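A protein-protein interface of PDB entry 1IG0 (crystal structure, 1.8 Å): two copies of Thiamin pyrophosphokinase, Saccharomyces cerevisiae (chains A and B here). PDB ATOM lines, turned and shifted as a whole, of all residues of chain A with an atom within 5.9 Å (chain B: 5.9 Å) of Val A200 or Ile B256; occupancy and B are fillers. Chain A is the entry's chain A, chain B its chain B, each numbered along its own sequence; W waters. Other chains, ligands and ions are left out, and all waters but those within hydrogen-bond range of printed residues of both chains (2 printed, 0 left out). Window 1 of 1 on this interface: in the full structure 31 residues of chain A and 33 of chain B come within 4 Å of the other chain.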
ATOM      1  N   GLY A 191      -5.587  -8.333   9.860  1.00  0.00           N
ATOM      2  CA  GLY A 191      -6.149  -6.994   9.894  1.00  0.00           C
ATOM      3  C   GLY A 191      -5.105  -5.894   9.915  1.00  0.00           C
ATOM      4  O   GLY A 191      -5.443  -4.710   9.853  1.00  0.00           O
ATOM      5  N   ARG A 195      -3.388  -3.171   3.011  1.00  0.00           N
ATOM      6  CA  ARG A 195      -3.902  -1.884   2.543  1.00  0.00           C
ATOM      7  C   ARG A 195      -3.950  -1.029   3.803  1.00  0.00           C
ATOM      8  O   ARG A 195      -4.604  -1.395   4.777  1.00  0.00           O
ATOM      9  CB  ARG A 195      -5.295  -2.075   1.931  1.00  0.00           C
ATOM     10  CG  ARG A 195      -5.262  -3.047   0.745  1.00  0.00           C
ATOM     11  CD  ARG A 195      -6.644  -3.532   0.278  1.00  0.00           C
ATOM     12  NE  ARG A 195      -7.293  -2.602  -0.649  1.00  0.00           N
ATOM     13  CZ  ARG A 195      -8.337  -1.814  -0.362  1.00  0.00           C
ATOM     14  NH1 ARG A 195      -8.908  -1.799   0.849  1.00  0.00           N
ATOM     15  NH2 ARG A 195      -8.838  -1.044  -1.317  1.00  0.00           N
ATOM     16  N   PHE A 196      -3.248   0.098   3.797  1.00  0.00           N
ATOM     17  CA  PHE A 196      -3.184   0.929   4.991  1.00  0.00           C
ATOM     18  C   PHE A 196      -4.498   1.419   5.582  1.00  0.00           C
ATOM     19  O   PHE A 196      -4.649   1.426   6.803  1.00  0.00           O
ATOM     20  CB  PHE A 196      -2.252   2.123   4.774  1.00  0.00           C
ATOM     21  CG  PHE A 196      -1.726   2.703   6.055  1.00  0.00           C
ATOM     22  CD1 PHE A 196      -1.019   1.902   6.948  1.00  0.00           C
ATOM     23  CD2 PHE A 196      -1.959   4.033   6.389  1.00  0.00           C
ATOM     24  CE1 PHE A 196      -0.556   2.413   8.158  1.00  0.00           C
ATOM     25  CE2 PHE A 196      -1.498   4.556   7.599  1.00  0.00           C
ATOM     26  CZ  PHE A 196      -0.794   3.743   8.485  1.00  0.00           C
ATOM     27  N   ASP A 197      -5.448   1.834   4.752  1.00  0.00           N
ATOM     28  CA  ASP A 197      -6.708   2.306   5.313  1.00  0.00           C
ATOM     29  C   ASP A 197      -7.399   1.177   6.072  1.00  0.00           C
ATOM     30  O   ASP A 197      -8.200   1.424   6.975  1.00  0.00           O
ATOM     31  CB  ASP A 197      -7.623   2.881   4.223  1.00  0.00           C
ATOM     32  CG  ASP A 197      -7.964   1.877   3.148  1.00  0.00           C
ATOM     33  OD1 ASP A 197      -7.036   1.332   2.517  1.00  0.00           O
ATOM     34  OD2 ASP A 197      -9.170   1.642   2.928  1.00  0.00           O
ATOM     35  N   GLN A 198      -7.078  -0.064   5.714  1.00  0.00           N
ATOM     36  CA  GLN A 198      -7.654  -1.216   6.396  1.00  0.00           C
ATOM     37  C   GLN A 198      -6.984  -1.393   7.752  1.00  0.00           C
ATOM     38  O   GLN A 198      -7.627  -1.795   8.718  1.00  0.00           O
ATOM     39  CB  GLN A 198      -7.486  -2.490   5.565  1.00  0.00           C
ATOM     40  CG  GLN A 198      -8.520  -2.645   4.465  1.00  0.00           C
ATOM     41  CD  GLN A 198      -9.941  -2.495   4.983  1.00  0.00           C
ATOM     42  OE1 GLN A 198     -10.321  -3.116   5.976  1.00  0.00           O
ATOM     43  NE2 GLN A 198     -10.733  -1.668   4.309  1.00  0.00           N
ATOM     44  N   THR A 199      -5.689  -1.103   7.820  1.00  0.00           N
ATOM     45  CA  THR A 199      -4.965  -1.204   9.080  1.00  0.00           C
ATOM     46  C   THR A 199      -5.587  -0.211  10.055  1.00  0.00           C
ATOM     47  O   THR A 199      -5.817  -0.525  11.220  1.00  0.00           O
ATOM     48  CB  THR A 199      -3.466  -0.854   8.912  1.00  0.00           C
ATOM     49  OG1 THR A 199      -2.798  -1.922   8.230  1.00  0.00           O
ATOM     50  CG2 THR A 199      -2.808  -0.625  10.270  1.00  0.00           C
ATOM     51  N   VAL A 200      -5.864   0.993   9.567  1.00  0.00           N
ATOM     52  CA  VAL A 200      -6.460   2.025  10.405  1.00  0.00           C
ATOM     53  C   VAL A 200      -7.866   1.615  10.844  1.00  0.00           C
ATOM     54  O   VAL A 200      -8.236   1.811  11.997  1.00  0.00           O
ATOM     55  CB  VAL A 200      -6.537   3.373   9.661  1.00  0.00           C
ATOM     56  CG1 VAL A 200      -7.343   4.378  10.471  1.00  0.00           C
ATOM     57  CG2 VAL A 200      -5.139   3.905   9.405  1.00  0.00           C
ATOM     58  N   HIS A 201      -8.651   1.050   9.931  1.00  0.00           N
ATOM     59  CA  HIS A 201      -9.990   0.638  10.301  1.00  0.00           C
ATOM     60  C   HIS A 201      -9.952  -0.425  11.396  1.00  0.00           C
ATOM     61  O   HIS A 201     -10.765  -0.412  12.324  1.00  0.00           O
ATOM     62  CB  HIS A 201     -10.783   0.106   9.103  1.00  0.00           C
ATOM     63  CG  HIS A 201     -12.149  -0.393   9.484  1.00  0.00           C
ATOM     64  ND1 HIS A 201     -12.433  -1.730   9.664  1.00  0.00           N
ATOM     65  CD2 HIS A 201     -13.284   0.274   9.819  1.00  0.00           C
ATOM     66  CE1 HIS A 201     -13.678  -1.867  10.093  1.00  0.00           C
ATOM     67  NE2 HIS A 201     -14.214  -0.665  10.195  1.00  0.00           N
ATOM     68  N   SER A 202      -9.009  -1.352  11.281  1.00  0.00           N
ATOM     69  CA  SER A 202      -8.872  -2.409  12.275  1.00  0.00           C
ATOM     70  C   SER A 202      -8.639  -1.773  13.635  1.00  0.00           C
ATOM     71  O   SER A 202      -9.222  -2.191  14.634  1.00  0.00           O
ATOM     72  CB  SER A 202      -7.702  -3.337  11.933  1.00  0.00           C
ATOM     73  OG  SER A 202      -7.985  -4.104  10.775  1.00  0.00           O
ATOM     74  N   ILE A 203      -7.795  -0.749  13.670  1.00  0.00           N
ATOM     75  CA  ILE A 203      -7.507  -0.063  14.921  1.00  0.00           C
ATOM     76  C   ILE A 203      -8.768   0.585  15.494  1.00  0.00           C
ATOM     77  O   ILE A 203      -8.982   0.564  16.707  1.00  0.00           O
ATOM     78  CB  ILE A 203      -6.410   1.015  14.731  1.00  0.00           C
ATOM     79  CG1 ILE A 203      -5.083   0.346  14.350  1.00  0.00           C
ATOM     80  CG2 ILE A 203      -6.237   1.818  16.013  1.00  0.00           C
ATOM     81  CD1 ILE A 203      -4.565  -0.638  15.389  1.00  0.00           C
ATOM     82  N   THR A 204      -9.609   1.149  14.631  1.00  0.00           N
ATOM     83  CA  THR A 204     -10.834   1.782  15.106  1.00  0.00           C
ATOM     84  C   THR A 204     -11.724   0.761  15.808  1.00  0.00           C
ATOM     85  O   THR A 204     -12.436   1.098  16.754  1.00  0.00           O
ATOM     86  CB  THR A 204     -11.650   2.431  13.958  1.00  0.00           C
ATOM     87  OG1 THR A 204     -12.257   1.412  13.155  1.00  0.00           O
ATOM     88  CG2 THR A 204     -10.753   3.300  13.090  1.00  0.00           C
ATOM     89  N   GLN A 205     -11.678  -0.488  15.349  1.00  0.00           N
ATOM     90  CA  GLN A 205     -12.486  -1.547  15.950  1.00  0.00           C
ATOM     91  C   GLN A 205     -12.142  -1.734  17.423  1.00  0.00           C
ATOM     92  O   GLN A 205     -13.013  -2.032  18.239  1.00  0.00           O
ATOM     93  CB  GLN A 205     -12.283  -2.874  15.209  1.00  0.00           C
ATOM     94  CG  GLN A 205     -12.952  -2.970  13.837  1.00  0.00           C
ATOM     95  CD  GLN A 205     -14.472  -2.946  13.910  1.00  0.00           C
ATOM     96  OE1 GLN A 205     -15.065  -3.351  14.911  1.00  0.00           O
ATOM     97  NE2 GLN A 205     -15.110  -2.492  12.835  1.00  0.00           N
ATOM     98  N   ILE A 256      -3.321   6.147  19.340  1.00  0.00           N
ATOM     99  CA  ILE A 256      -3.789   6.277  17.970  1.00  0.00           C
ATOM    100  C   ILE A 256      -5.137   6.976  17.861  1.00  0.00           C
ATOM    101  O   ILE A 256      -6.102   6.598  18.523  1.00  0.00           O
ATOM    102  CB  ILE A 256      -3.867   4.889  17.293  1.00  0.00           C
ATOM    103  CG1 ILE A 256      -2.523   4.170  17.446  1.00  0.00           C
ATOM    104  CG2 ILE A 256      -4.214   5.041  15.815  1.00  0.00           C
ATOM    105  CD1 ILE A 256      -2.507   2.754  16.883  1.00  0.00           C
ATOM    106  N   GLY A 257      -5.184   8.010  17.026  1.00  0.00           N
ATOM    107  CA  GLY A 257      -6.417   8.748  16.814  1.00  0.00           C
ATOM    108  C   GLY A 257      -6.803   9.770  17.869  1.00  0.00           C
ATOM    109  O   GLY A 257      -7.695  10.589  17.640  1.00  0.00           O
ATOM    110  N   GLU A 258      -6.138   9.740  19.019  1.00  0.00           N
ATOM    111  CA  GLU A 258      -6.463  10.673  20.089  1.00  0.00           C
ATOM    112  C   GLU A 258      -5.330  10.827  21.099  1.00  0.00           C
ATOM    113  O   GLU A 258      -4.797   9.840  21.603  1.00  0.00           O
ATOM    114  CB  GLU A 258      -7.727  10.189  20.801  1.00  0.00           C
ATOM    115  CG  GLU A 258      -8.200  11.056  21.946  1.00  0.00           C
ATOM    116  CD  GLU A 258      -9.401  10.455  22.653  1.00  0.00           C
ATOM    117  OE1 GLU A 258      -9.257   9.383  23.281  1.00  0.00           O
ATOM    118  OE2 GLU A 258     -10.492  11.054  22.574  1.00  0.00           O
ATOM    119  N   VAL A 279       0.299  11.288  18.804  1.00  0.00           N
ATOM    120  CA  VAL A 279       0.880  10.952  17.511  1.00  0.00           C
ATOM    121  C   VAL A 279       1.229  12.238  16.769  1.00  0.00           C
ATOM    122  O   VAL A 279       2.187  12.286  15.997  1.00  0.00           O
ATOM    123  CB  VAL A 279      -0.110  10.126  16.660  1.00  0.00           C
ATOM    124  CG1 VAL A 279       0.364  10.049  15.214  1.00  0.00           C
ATOM    125  CG2 VAL A 279      -0.234   8.732  17.240  1.00  0.00           C
ATOM    126  N   VAL A 280       0.451  13.283  17.022  1.00  0.00           N
ATOM    127  CA  VAL A 280       0.657  14.575  16.378  1.00  0.00           C
ATOM    128  C   VAL A 280       1.925  15.280  16.854  1.00  0.00           C
ATOM    129  O   VAL A 280       2.630  15.898  16.057  1.00  0.00           O
ATOM    130  CB  VAL A 280      -0.554  15.506  16.615  1.00  0.00           C
ATOM    131  CG1 VAL A 280      -0.339  16.843  15.916  1.00  0.00           C
ATOM    132  CG2 VAL A 280      -1.823  14.838  16.103  1.00  0.00           C
ATOM    133  N   ILE B 203       4.190   7.354  11.204  1.00  0.00           N
ATOM    134  CA  ILE B 203       3.070   8.265  11.019  1.00  0.00           C
ATOM    135  C   ILE B 203       3.292   9.580  11.763  1.00  0.00           C
ATOM    136  O   ILE B 203       2.936  10.643  11.260  1.00  0.00           O
ATOM    137  CB  ILE B 203       1.739   7.633  11.486  1.00  0.00           C
ATOM    138  CG1 ILE B 203       1.408   6.418  10.612  1.00  0.00           C
ATOM    139  CG2 ILE B 203       0.617   8.661  11.411  1.00  0.00           C
ATOM    140  CD1 ILE B 203       1.349   6.722   9.130  1.00  0.00           C
ATOM    141  N   TYR B 207       3.330  14.233  10.802  1.00  0.00           N
ATOM    142  CA  TYR B 207       2.816  15.357  11.579  1.00  0.00           C
ATOM    143  C   TYR B 207       3.921  16.266  12.115  1.00  0.00           C
ATOM    144  O   TYR B 207       3.855  17.486  11.959  1.00  0.00           O
ATOM    145  CB  TYR B 207       1.974  14.862  12.759  1.00  0.00           C
ATOM    146  CG  TYR B 207       0.631  14.265  12.387  1.00  0.00           C
ATOM    147  CD1 TYR B 207       0.438  12.886  12.377  1.00  0.00           C
ATOM    148  CD2 TYR B 207      -0.456  15.086  12.072  1.00  0.00           C
ATOM    149  CE1 TYR B 207      -0.806  12.332  12.066  1.00  0.00           C
ATOM    150  CE2 TYR B 207      -1.705  14.542  11.759  1.00  0.00           C
ATOM    151  CZ  TYR B 207      -1.873  13.165  11.760  1.00  0.00           C
ATOM    152  OH  TYR B 207      -3.108  12.627  11.468  1.00  0.00           O
ATOM    153  N   LEU B 254      -7.456   9.351   6.734  1.00  0.00           N
ATOM    154  CA  LEU B 254      -7.128   8.848   8.062  1.00  0.00           C
ATOM    155  C   LEU B 254      -6.728   9.877   9.113  1.00  0.00           C
ATOM    156  O   LEU B 254      -5.633  10.438   9.055  1.00  0.00           O
ATOM    157  CB  LEU B 254      -6.006   7.821   7.914  1.00  0.00           C
ATOM    158  CG  LEU B 254      -6.136   6.959   6.650  1.00  0.00           C
ATOM    159  CD1 LEU B 254      -4.869   6.144   6.439  1.00  0.00           C
ATOM    160  CD2 LEU B 254      -7.357   6.051   6.765  1.00  0.00           C
ATOM    161  N   PRO B 255      -7.609  10.126  10.097  1.00  0.00           N
ATOM    162  CA  PRO B 255      -7.332  11.088  11.167  1.00  0.00           C
ATOM    163  C   PRO B 255      -6.542  10.403  12.280  1.00  0.00           C
ATOM    164  O   PRO B 255      -6.984  10.338  13.427  1.00  0.00           O
ATOM    165  CB  PRO B 255      -8.728  11.503  11.611  1.00  0.00           C
ATOM    166  CG  PRO B 255      -9.480  10.212  11.509  1.00  0.00           C
ATOM    167  CD  PRO B 255      -9.013   9.673  10.159  1.00  0.00           C
ATOM    168  N   ILE B 256      -5.372   9.888  11.924  1.00  0.00           N
ATOM    169  CA  ILE B 256      -4.515   9.192  12.872  1.00  0.00           C
ATOM    170  C   ILE B 256      -3.913  10.173  13.873  1.00  0.00           C
ATOM    171  O   ILE B 256      -3.318  11.176  13.489  1.00  0.00           O
ATOM    172  CB  ILE B 256      -3.371   8.461  12.136  1.00  0.00           C
ATOM    173  CG1 ILE B 256      -3.939   7.655  10.966  1.00  0.00           C
ATOM    174  CG2 ILE B 256      -2.629   7.536  13.100  1.00  0.00           C
ATOM    175  CD1 ILE B 256      -2.875   7.009  10.088  1.00  0.00           C
ATOM    176  N   GLY B 257      -4.081   9.891  15.160  1.00  0.00           N
ATOM    177  CA  GLY B 257      -3.521  10.769  16.174  1.00  0.00           C
ATOM    178  C   GLY B 257      -4.442  11.843  16.723  1.00  0.00           C
ATOM    179  O   GLY B 257      -4.318  12.231  17.886  1.00  0.00           O
ATOM    180  N   GLU B 258      -5.359  12.340  15.901  1.00  0.00           N
ATOM    181  CA  GLU B 258      -6.279  13.368  16.368  1.00  0.00           C
ATOM    182  C   GLU B 258      -7.521  13.487  15.491  1.00  0.00           C
ATOM    183  O   GLU B 258      -7.431  13.515  14.264  1.00  0.00           O
ATOM    184  CB  GLU B 258      -5.547  14.717  16.469  1.00  0.00           C
ATOM    185  CG  GLU B 258      -5.877  15.751  15.400  1.00  0.00           C
ATOM    186  CD  GLU B 258      -5.129  17.058  15.617  1.00  0.00           C
ATOM    187  OE1 GLU B 258      -4.965  17.461  16.788  1.00  0.00           O
ATOM    188  OE2 GLU B 258      -4.711  17.689  14.623  1.00  0.00           O
ATOM    189  N   VAL B 279     -10.744   8.157  14.674  1.00  0.00           N
ATOM    190  CA  VAL B 279     -10.407   6.744  14.791  1.00  0.00           C
ATOM    191  C   VAL B 279     -11.113   6.147  16.004  1.00  0.00           C
ATOM    192  O   VAL B 279     -11.453   4.964  16.018  1.00  0.00           O
ATOM    193  CB  VAL B 279      -8.877   6.546  14.951  1.00  0.00           C
ATOM    194  CG1 VAL B 279      -8.562   5.097  15.320  1.00  0.00           C
ATOM    195  CG2 VAL B 279      -8.171   6.925  13.660  1.00  0.00           C
ATOM    196  N   VAL B 284     -14.367   6.826   9.980  1.00  0.00           N
ATOM    197  CA  VAL B 284     -13.213   7.005   9.108  1.00  0.00           C
ATOM    198  C   VAL B 284     -13.560   6.558   7.695  1.00  0.00           C
ATOM    199  O   VAL B 284     -14.071   5.456   7.493  1.00  0.00           O
ATOM    200  CB  VAL B 284     -12.009   6.171   9.602  1.00  0.00           C
ATOM    201  CG1 VAL B 284     -10.853   6.284   8.622  1.00  0.00           C
ATOM    202  CG2 VAL B 284     -11.579   6.646  10.979  1.00  0.00           C
ATOM    203  N   ILE B 305      -4.023  12.312   7.436  1.00  0.00           N
ATOM    204  CA  ILE B 305      -3.180  11.426   6.649  1.00  0.00           C
ATOM    205  C   ILE B 305      -4.027  10.805   5.549  1.00  0.00           C
ATOM    206  O   ILE B 305      -5.169  10.410   5.783  1.00  0.00           O
ATOM    207  CB  ILE B 305      -2.592  10.289   7.506  1.00  0.00           C
ATOM    208  CG1 ILE B 305      -1.838  10.874   8.705  1.00  0.00           C
ATOM    209  CG2 ILE B 305      -1.667   9.424   6.658  1.00  0.00           C
ATOM    210  CD1 ILE B 305      -0.690  11.800   8.330  1.00  0.00           C
HETATM  211  O   HOH W   1      -8.912  10.363  15.240  1.00  0.00           O
HETATM  212  O   HOH W   2      -2.445  11.048  19.229  1.00  0.00           O
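The backbone NH (N) of Gly A257 sits close to the backbone NH (N) of Gly B257 (2.9 Å). The backbone carbonyl oxygen of Gly B257 lies within hydrogen-bond range of the backbone NH of Glu A258, at 3.3 Å. The backbone carbonyl oxygen of Gly A257 lies close to the backbone NH of Glu B258, 3.4 Å away.
The side-chain hydroxyl (OG1) of Thr A204 lies within hydrogen-bond range of the backbone carbonyl oxygen (O) of His A201, at 2.5 Å. The side-chain hydroxyl (OH) of Tyr B207 sits at hydrogen-bond distance from the backbone carbonyl oxygen (O) of Ile B256, at 2.5 Å. N of Leu B254 is in hydrogen-bond range of O of Ile B305 (2.7 Å).
Ile B203 touches Phe A196 (CD1 to CZ, 3.7 Å). Phe A196 touches Leu B254. Ile B256 touches Phe A196 (CD1 to CE2, 3.8 Å). Val A200 touches Leu B254. CG2 of Val A200 touches CD1 of Ile B256, 3.9 Å away. Val B279 touches Thr A204. CA of Gly A257 touches O of Pro B255 (3.8 Å). Val B279 touches Gly A257 (CB to CA, 3.8 Å). Val A280 touches Tyr B207 (O to CB, 3.5 Å). Glu B258 touches Val A280 (CB to CG2, 3.7 Å).
Arg A195 touches none of the printed residues of chain B. Of the printed residues of chain B, Phe A196 touches Ile B203 (3.7 Å), Leu B254 (3.6 Å) and Ile B256 (3.8 Å). Printed residues of chain B within 4 Å of Val A200: Leu B254 (3.7 Å) and Ile B256 (3.9 Å). Of the printed residues of chain B, Glu A258 touches Gly B257 (3.3 Å). Of the printed residues of chain B, Val A279 touches Gly B257. Of the printed residues of chain A, Gly B257 touches Gly A257 (2.9 Å), Glu A258 (3.3 Å) and Val A279 (3.5 Å). The nearest printed residue of chain A that does not touch Ile B256 is Ile A256 (4.01 Å). The nearest printed residue of chain A that does not touch Gly B257 is Val A280 (4.02 Å).
Hydrophobic or aromatic side chains of chain B within 4 Å of the printed part of chain A: Ile B203, Tyr B207, Leu B254, Ile B256 and Val B279. Of the 17 printed residues of chain A, 7 touch a printed residue of chain B. Hydrophobic or aromatic side chains of chain A within 4 Å of the printed part of chain B: Phe A196, Val A200, Val A279 and Val A280. Among the printed residues, no Asp or Glu carboxylate lies within 4 Å of a Lys or Arg side-chain nitrogen of the other chain.
Gly B257 touches its own counterpart, Gly A257. Gly A257 touches Glu B258, and with the chains exchanged Glu A258 touches Gly B257. Gly A257 touches Val B279, and with the chains exchanged Val A279 touches Gly B257. Of the 14 pairs that touch across the chains among the printed residues, 5 have their exchanged pair printed and touching as well.
Water W2 bridges O of Gly B257 (2.6 Å) and N of Val A279 (2.8 Å). Water W1 lies within hydrogen-bond range of O of Pro B255 (2.6 Å), O of Gly A257 (2.7 Å) and N of Val B279 (2.9 Å).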
